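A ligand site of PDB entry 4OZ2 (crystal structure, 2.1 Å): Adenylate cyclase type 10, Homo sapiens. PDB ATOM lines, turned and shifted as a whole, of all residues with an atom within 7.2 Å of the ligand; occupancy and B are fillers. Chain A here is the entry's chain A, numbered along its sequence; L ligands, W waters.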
ATOM      1  N   PHE A  97       2.721  16.075   9.305  1.00  0.00           N
ATOM      2  CA  PHE A  97       1.914  14.908   8.895  1.00  0.00           C
ATOM      3  C   PHE A  97       0.675  14.857   9.774  1.00  0.00           C
ATOM      4  O   PHE A  97       0.752  15.154  10.950  1.00  0.00           O
ATOM      5  CB  PHE A  97       2.684  13.575   8.989  1.00  0.00           C
ATOM      6  CG  PHE A  97       3.901  13.478   8.093  1.00  0.00           C
ATOM      7  CD1 PHE A  97       5.123  14.024   8.486  1.00  0.00           C
ATOM      8  CD2 PHE A  97       3.828  12.835   6.851  1.00  0.00           C
ATOM      9  CE1 PHE A  97       6.251  13.957   7.656  1.00  0.00           C
ATOM     10  CE2 PHE A  97       4.950  12.744   6.023  1.00  0.00           C
ATOM     11  CZ  PHE A  97       6.155  13.322   6.426  1.00  0.00           C
ATOM     12  N   ALA A  98      -0.454  14.475   9.208  1.00  0.00           N
ATOM     13  CA  ALA A  98      -1.667  14.245  10.007  1.00  0.00           C
ATOM     14  C   ALA A  98      -2.405  13.102   9.350  1.00  0.00           C
ATOM     15  O   ALA A  98      -3.106  13.298   8.361  1.00  0.00           O
ATOM     16  CB  ALA A  98      -2.528  15.511  10.032  1.00  0.00           C
ATOM     17  N   GLY A  99      -2.230  11.916   9.914  1.00  0.00           N
ATOM     18  CA  GLY A  99      -2.723  10.660   9.367  1.00  0.00           C
ATOM     19  C   GLY A  99      -2.051  10.229   8.073  1.00  0.00           C
ATOM     20  O   GLY A  99      -0.857   9.895   8.042  1.00  0.00           O
ATOM     21  N   ASP A 100      -2.841  10.223   7.007  1.00  0.00           N
ATOM     22  CA  ASP A 100      -2.460   9.937   5.622  1.00  0.00           C
ATOM     23  C   ASP A 100      -2.527  11.243   4.810  1.00  0.00           C
ATOM     24  O   ASP A 100      -2.880  11.226   3.634  1.00  0.00           O
ATOM     25  CB  ASP A 100      -3.437   8.887   5.038  1.00  0.00           C
ATOM     26  CG  ASP A 100      -4.907   9.155   5.360  1.00  0.00           C
ATOM     27  OD1 ASP A 100      -5.403  10.240   4.971  1.00  0.00           O
ATOM     28  OD2 ASP A 100      -5.544   8.292   6.014  1.00  0.00           O
ATOM     29  N   PHE A 297     -10.302  16.260  21.331  1.00  0.00           N
ATOM     30  CA  PHE A 297     -10.010  17.141  20.211  1.00  0.00           C
ATOM     31  C   PHE A 297     -10.565  18.503  20.573  1.00  0.00           C
ATOM     32  O   PHE A 297     -11.781  18.676  20.631  1.00  0.00           O
ATOM     33  CB  PHE A 297     -10.565  16.573  18.886  1.00  0.00           C
ATOM     34  CG  PHE A 297      -9.608  16.651  17.703  1.00  0.00           C
ATOM     35  CD1 PHE A 297      -8.811  17.777  17.482  1.00  0.00           C
ATOM     36  CD2 PHE A 297      -9.508  15.581  16.797  1.00  0.00           C
ATOM     37  CE1 PHE A 297      -7.948  17.842  16.397  1.00  0.00           C
ATOM     38  CE2 PHE A 297      -8.665  15.650  15.704  1.00  0.00           C
ATOM     39  CZ  PHE A 297      -7.877  16.777  15.513  1.00  0.00           C
ATOM     40  N   ASN A 334      -0.759  15.496  20.576  1.00  0.00           N
ATOM     41  CA  ASN A 334      -0.156  14.808  19.432  1.00  0.00           C
ATOM     42  C   ASN A 334       0.092  15.772  18.241  1.00  0.00           C
ATOM     43  O   ASN A 334       1.119  15.678  17.583  1.00  0.00           O
ATOM     44  CB  ASN A 334      -0.996  13.563  19.053  1.00  0.00           C
ATOM     45  CG  ASN A 334      -0.521  12.859  17.804  1.00  0.00           C
ATOM     46  OD1 ASN A 334      -1.066  13.035  16.729  1.00  0.00           O
ATOM     47  ND2 ASN A 334       0.534  12.084  17.883  1.00  0.00           N
ATOM     48  N   LYS A 335      -0.850  16.690  17.957  1.00  0.00           N
ATOM     49  CA  LYS A 335      -0.749  17.673  16.868  1.00  0.00           C
ATOM     50  C   LYS A 335      -1.516  18.900  17.258  1.00  0.00           C
ATOM     51  O   LYS A 335      -2.439  18.838  18.068  1.00  0.00           O
ATOM     52  CB  LYS A 335      -1.409  17.177  15.554  1.00  0.00           C
ATOM     53  CG  LYS A 335      -0.838  15.947  14.887  1.00  0.00           C
ATOM     54  CD  LYS A 335       0.466  16.138  14.126  1.00  0.00           C
ATOM     55  CE  LYS A 335       0.991  14.726  13.989  1.00  0.00           C
ATOM     56  NZ  LYS A 335       2.401  14.668  13.600  1.00  0.00           N
ATOM     57  N   VAL A 336      -1.146  20.028  16.662  1.00  0.00           N
ATOM     58  CA  VAL A 336      -1.846  21.302  16.704  1.00  0.00           C
ATOM     59  C   VAL A 336      -1.859  21.759  15.241  1.00  0.00           C
ATOM     60  O   VAL A 336      -0.880  21.544  14.549  1.00  0.00           O
ATOM     61  CB  VAL A 336      -1.142  22.369  17.613  1.00  0.00           C
ATOM     62  CG1 VAL A 336      -2.046  23.573  17.831  1.00  0.00           C
ATOM     63  CG2 VAL A 336      -0.696  21.784  18.968  1.00  0.00           C
ATOM     64  N   PHE A 337      -2.934  22.364  14.781  1.00  0.00           N
ATOM     65  CA  PHE A 337      -3.065  22.891  13.414  1.00  0.00           C
ATOM     66  C   PHE A 337      -4.232  23.830  13.400  1.00  0.00           C
ATOM     67  O   PHE A 337      -5.039  23.809  14.329  1.00  0.00           O
ATOM     68  CB  PHE A 337      -3.247  21.758  12.355  1.00  0.00           C
ATOM     69  CG  PHE A 337      -4.362  20.805  12.687  1.00  0.00           C
ATOM     70  CD1 PHE A 337      -5.655  21.018  12.205  1.00  0.00           C
ATOM     71  CD2 PHE A 337      -4.129  19.681  13.484  1.00  0.00           C
ATOM     72  CE1 PHE A 337      -6.705  20.138  12.522  1.00  0.00           C
ATOM     73  CE2 PHE A 337      -5.173  18.809  13.806  1.00  0.00           C
ATOM     74  CZ  PHE A 337      -6.461  19.046  13.322  1.00  0.00           C
ATOM     75  N   PHE A 339      -7.866  24.936  11.731  1.00  0.00           N
ATOM     76  CA  PHE A 339      -9.073  24.300  11.183  1.00  0.00           C
ATOM     77  C   PHE A 339     -10.284  25.267  11.258  1.00  0.00           C
ATOM     78  O   PHE A 339     -10.823  25.509  12.352  1.00  0.00           O
ATOM     79  CB  PHE A 339      -9.355  22.972  11.911  1.00  0.00           C
ATOM     80  CG  PHE A 339     -10.299  21.984  11.257  1.00  0.00           C
ATOM     81  CD1 PHE A 339     -10.801  22.216   9.976  1.00  0.00           C
ATOM     82  CD2 PHE A 339     -10.686  20.828  11.917  1.00  0.00           C
ATOM     83  CE1 PHE A 339     -11.674  21.302   9.367  1.00  0.00           C
ATOM     84  CE2 PHE A 339     -11.558  19.913  11.308  1.00  0.00           C
ATOM     85  CZ  PHE A 339     -12.043  20.154  10.039  1.00  0.00           C
ATOM     86  N   SER A 344      -6.671  23.942  16.711  1.00  0.00           N
ATOM     87  CA  SER A 344      -7.106  22.618  17.127  1.00  0.00           C
ATOM     88  C   SER A 344      -5.969  21.799  17.772  1.00  0.00           C
ATOM     89  O   SER A 344      -4.923  21.625  17.183  1.00  0.00           O
ATOM     90  CB  SER A 344      -7.693  21.837  15.949  1.00  0.00           C
ATOM     91  OG  SER A 344      -8.799  22.476  15.331  1.00  0.00           O
ATOM     92  N   LEU A 346      -5.039  18.125  18.962  1.00  0.00           N
ATOM     93  CA  LEU A 346      -5.343  16.710  18.971  1.00  0.00           C
ATOM     94  C   LEU A 346      -4.692  16.147  20.229  1.00  0.00           C
ATOM     95  O   LEU A 346      -3.478  15.939  20.254  1.00  0.00           O
ATOM     96  CB  LEU A 346      -4.860  16.024  17.660  1.00  0.00           C
ATOM     97  CG  LEU A 346      -5.485  14.660  17.258  1.00  0.00           C
ATOM     98  CD1 LEU A 346      -4.911  14.148  15.937  1.00  0.00           C
ATOM     99  CD2 LEU A 346      -5.328  13.574  18.315  1.00  0.00           C
ATOM    100  N   THR A 406       2.063   9.770  14.564  1.00  0.00           N
ATOM    101  CA  THR A 406       0.719  10.170  14.221  1.00  0.00           C
ATOM    102  C   THR A 406      -0.285   9.129  14.739  1.00  0.00           C
ATOM    103  O   THR A 406       0.075   7.972  15.037  1.00  0.00           O
ATOM    104  CB  THR A 406       0.534  10.314  12.665  1.00  0.00           C
ATOM    105  OG1 THR A 406       1.750  10.682  12.009  1.00  0.00           O
ATOM    106  CG2 THR A 406      -0.505  11.312  12.306  1.00  0.00           C
ATOM    107  N   VAL A 407      -1.529   9.564  14.852  1.00  0.00           N
ATOM    108  CA  VAL A 407      -2.682   8.706  15.132  1.00  0.00           C
ATOM    109  C   VAL A 407      -3.605   8.643  13.924  1.00  0.00           C
ATOM    110  O   VAL A 407      -3.795   9.654  13.247  1.00  0.00           O
ATOM    111  CB  VAL A 407      -3.400   9.127  16.423  1.00  0.00           C
ATOM    112  CG1 VAL A 407      -2.460   8.936  17.596  1.00  0.00           C
ATOM    113  CG2 VAL A 407      -3.899  10.587  16.342  1.00  0.00           C
ATOM    114  N   ILE A 408      -4.149   7.468  13.627  1.00  0.00           N
ATOM    115  CA  ILE A 408      -5.085   7.294  12.509  1.00  0.00           C
ATOM    116  C   ILE A 408      -6.238   6.407  13.014  1.00  0.00           C
ATOM    117  O   ILE A 408      -6.007   5.392  13.676  1.00  0.00           O
ATOM    118  CB  ILE A 408      -4.444   6.640  11.244  1.00  0.00           C
ATOM    119  CG1 ILE A 408      -3.248   7.458  10.720  1.00  0.00           C
ATOM    120  CG2 ILE A 408      -5.510   6.387  10.083  1.00  0.00           C
ATOM    121  CD1 ILE A 408      -2.479   6.822   9.515  1.00  0.00           C
ATOM    122  N   GLY A 409      -7.452   6.794  12.689  1.00  0.00           N
ATOM    123  CA  GLY A 409      -8.583   5.907  12.950  1.00  0.00           C
ATOM    124  C   GLY A 409      -9.871   6.662  12.928  1.00  0.00           C
ATOM    125  O   GLY A 409      -9.873   7.883  13.055  1.00  0.00           O
ATOM    126  N   VAL A 412     -10.507   9.136  15.749  1.00  0.00           N
ATOM    127  CA  VAL A 412      -9.809  10.398  15.558  1.00  0.00           C
ATOM    128  C   VAL A 412     -10.680  11.319  14.709  1.00  0.00           C
ATOM    129  O   VAL A 412     -10.883  12.467  15.083  1.00  0.00           O
ATOM    130  CB  VAL A 412      -8.340  10.228  14.984  1.00  0.00           C
ATOM    131  CG1 VAL A 412      -7.661  11.586  14.809  1.00  0.00           C
ATOM    132  CG2 VAL A 412      -7.501   9.315  15.877  1.00  0.00           C
ATOM    133  N   ASN A 413     -11.193  10.804  13.560  1.00  0.00           N
ATOM    134  CA  ASN A 413     -12.036  11.624  12.652  1.00  0.00           C
ATOM    135  C   ASN A 413     -13.342  12.026  13.351  1.00  0.00           C
ATOM    136  O   ASN A 413     -13.797  13.165  13.184  1.00  0.00           O
ATOM    137  CB  ASN A 413     -12.371  10.878  11.303  1.00  0.00           C
ATOM    138  CG  ASN A 413     -11.188  10.235  10.626  1.00  0.00           C
ATOM    139  OD1 ASN A 413     -10.052  10.703  10.709  1.00  0.00           O
ATOM    140  ND2 ASN A 413     -11.410   9.120   9.957  1.00  0.00           N
ATOM    141  N   LEU A 414     -13.946  11.100  14.121  1.00  0.00           N
ATOM    142  CA  LEU A 414     -15.168  11.365  14.873  1.00  0.00           C
ATOM    143  C   LEU A 414     -14.982  12.530  15.874  1.00  0.00           C
ATOM    144  O   LEU A 414     -15.780  13.460  15.842  1.00  0.00           O
ATOM    145  CB  LEU A 414     -15.703  10.092  15.576  1.00  0.00           C
ATOM    146  CG  LEU A 414     -16.999  10.283  16.420  1.00  0.00           C
ATOM    147  CD1 LEU A 414     -18.146  10.777  15.556  1.00  0.00           C
ATOM    148  CD2 LEU A 414     -17.370   9.060  17.199  1.00  0.00           C
ATOM    149  N   ALA A 415     -13.963  12.489  16.757  1.00  0.00           N
ATOM    150  CA  ALA A 415     -13.702  13.606  17.691  1.00  0.00           C
ATOM    151  C   ALA A 415     -13.544  14.971  16.989  1.00  0.00           C
ATOM    152  O   ALA A 415     -14.084  15.974  17.472  1.00  0.00           O
ATOM    153  CB  ALA A 415     -12.485  13.326  18.545  1.00  0.00           C
ATOM    154  N   ALA A 416     -12.810  14.992  15.825  1.00  0.00           N
ATOM    155  CA  ALA A 416     -12.661  16.149  14.947  1.00  0.00           C
ATOM    156  C   ALA A 416     -14.001  16.620  14.393  1.00  0.00           C
ATOM    157  O   ALA A 416     -14.282  17.821  14.426  1.00  0.00           O
ATOM    158  CB  ALA A 416     -11.673  15.839  13.805  1.00  0.00           C
ATOM    159  N   ARG A 417     -14.844  15.701  13.891  1.00  0.00           N
ATOM    160  CA  ARG A 417     -16.165  16.132  13.383  1.00  0.00           C
ATOM    161  C   ARG A 417     -17.048  16.627  14.502  1.00  0.00           C
ATOM    162  O   ARG A 417     -17.744  17.599  14.292  1.00  0.00           O
ATOM    163  CB  ARG A 417     -16.892  15.049  12.550  1.00  0.00           C
ATOM    164  CG  ARG A 417     -16.068  14.412  11.420  1.00  0.00           C
ATOM    165  CD  ARG A 417     -15.703  15.361  10.286  1.00  0.00           C
ATOM    166  NE  ARG A 417     -14.779  14.737   9.340  1.00  0.00           N
ATOM    167  CZ  ARG A 417     -13.830  15.389   8.666  1.00  0.00           C
ATOM    168  NH1 ARG A 417     -13.661  16.690   8.835  1.00  0.00           N
ATOM    169  NH2 ARG A 417     -13.035  14.729   7.827  1.00  0.00           N
ATOM    170  N   MET A 419     -16.211  18.258  17.453  1.00  0.00           N
ATOM    171  CA  MET A 419     -15.875  19.633  17.834  1.00  0.00           C
ATOM    172  C   MET A 419     -16.307  20.670  16.770  1.00  0.00           C
ATOM    173  O   MET A 419     -16.574  21.800  17.129  1.00  0.00           O
ATOM    174  CB  MET A 419     -14.395  19.799  18.237  1.00  0.00           C
ATOM    175  CG  MET A 419     -13.470  20.132  17.059  1.00  0.00           C
ATOM    176  SD  MET A 419     -11.716  19.795  17.309  1.00  0.00           S
ATOM    177  CE  MET A 419     -11.251  19.924  15.626  1.00  0.00           C
ATOM    178  N   MET A 420     -16.399  20.280  15.480  1.00  0.00           N
ATOM    179  CA  MET A 420     -16.813  21.216  14.434  1.00  0.00           C
ATOM    180  C   MET A 420     -18.322  21.324  14.287  1.00  0.00           C
ATOM    181  O   MET A 420     -18.821  22.409  14.036  1.00  0.00           O
ATOM    182  CB  MET A 420     -16.131  20.922  13.077  1.00  0.00           C
ATOM    183  CG  MET A 420     -14.582  20.990  13.130  1.00  0.00           C
ATOM    184  SD  MET A 420     -13.873  22.442  14.006  1.00  0.00           S
ATOM    185  CE  MET A 420     -14.441  23.803  12.899  1.00  0.00           C
HETATM  186  C1  LIG L   1      -4.325  15.314  12.808  1.00  0.00           C
HETATM  187  C2  LIG L   1      -4.843  13.965  12.443  1.00  0.00           C
HETATM  188  N1  LIG L   1      -4.840  11.850  12.194  1.00  0.00           N
HETATM  189  C3  LIG L   1      -6.048  12.240  11.769  1.00  0.00           C
HETATM  190  C4  LIG L   1      -6.090  13.602  11.925  1.00  0.00           C
HETATM  191  C5  LIG L   1      -7.245  14.464  11.583  1.00  0.00           C
HETATM  192  C6  LIG L   1      -9.595  14.746  11.145  1.00  0.00           C
HETATM  193  C7  LIG L   1      -9.375  16.076  10.966  1.00  0.00           C
HETATM  194  C8  LIG L   1      -8.144  16.645  11.090  1.00  0.00           C
HETATM  195  C9  LIG L   1      -7.069  15.831  11.390  1.00  0.00           C
HETATM  196  N2  LIG L   1      -4.074  12.890  12.618  1.00  0.00           N
HETATM  197  C10 LIG L   1      -8.522  13.921  11.465  1.00  0.00           C
HETATM  198  F1  LIG L   1     -10.430  16.880  10.662  1.00  0.00           F
HETATM  199  O   HOH W   1      -1.800  12.995  14.152  1.00  0.00           O
HETATM  200  O   HOH W   2      -6.072  17.811   8.682  1.00  0.00           O
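A nitrogen (N1) of the ligand lies within hydrogen-bond range of the backbone carbonyl oxygen of Val 407 (2.7 Å). The backbone NH of Gly 99 sits at hydrogen-bond distance from a nitrogen (N2) of the ligand, 3.4 Å away.
O of Phe 337 sits at hydrogen-bond distance from N of Ser 344, at 2.9 Å. N of Leu 346 sits at hydrogen-bond distance from O of Lys 335 (2.8 Å). The backbone NH (N) of Asn 334 is in hydrogen-bond range of the backbone carbonyl oxygen (O) of Leu 346 (2.8 Å).
Merely in contact with the ligand: Phe 339 (3.3 Å), Ala 98 (3.3 Å), Leu 346 (3.4 Å), Val 412 (3.5 Å), Ala 416 (3.5 Å), Asn 413 (3.6 Å), Phe 337 (3.7 Å), Arg 417 (3.7 Å) and Thr 406 (3.9 Å). Hydrophobic or aromatic side chains that line the ligand: Ala 98, Phe 337, Phe 339, Leu 346, Val 412 and Ala 416. The nearest printed residue that does not touch the ligand is Lys 335 (4.1 Å).
Water W1 bridges OD1 of Asn 334 and N2 of the ligand.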
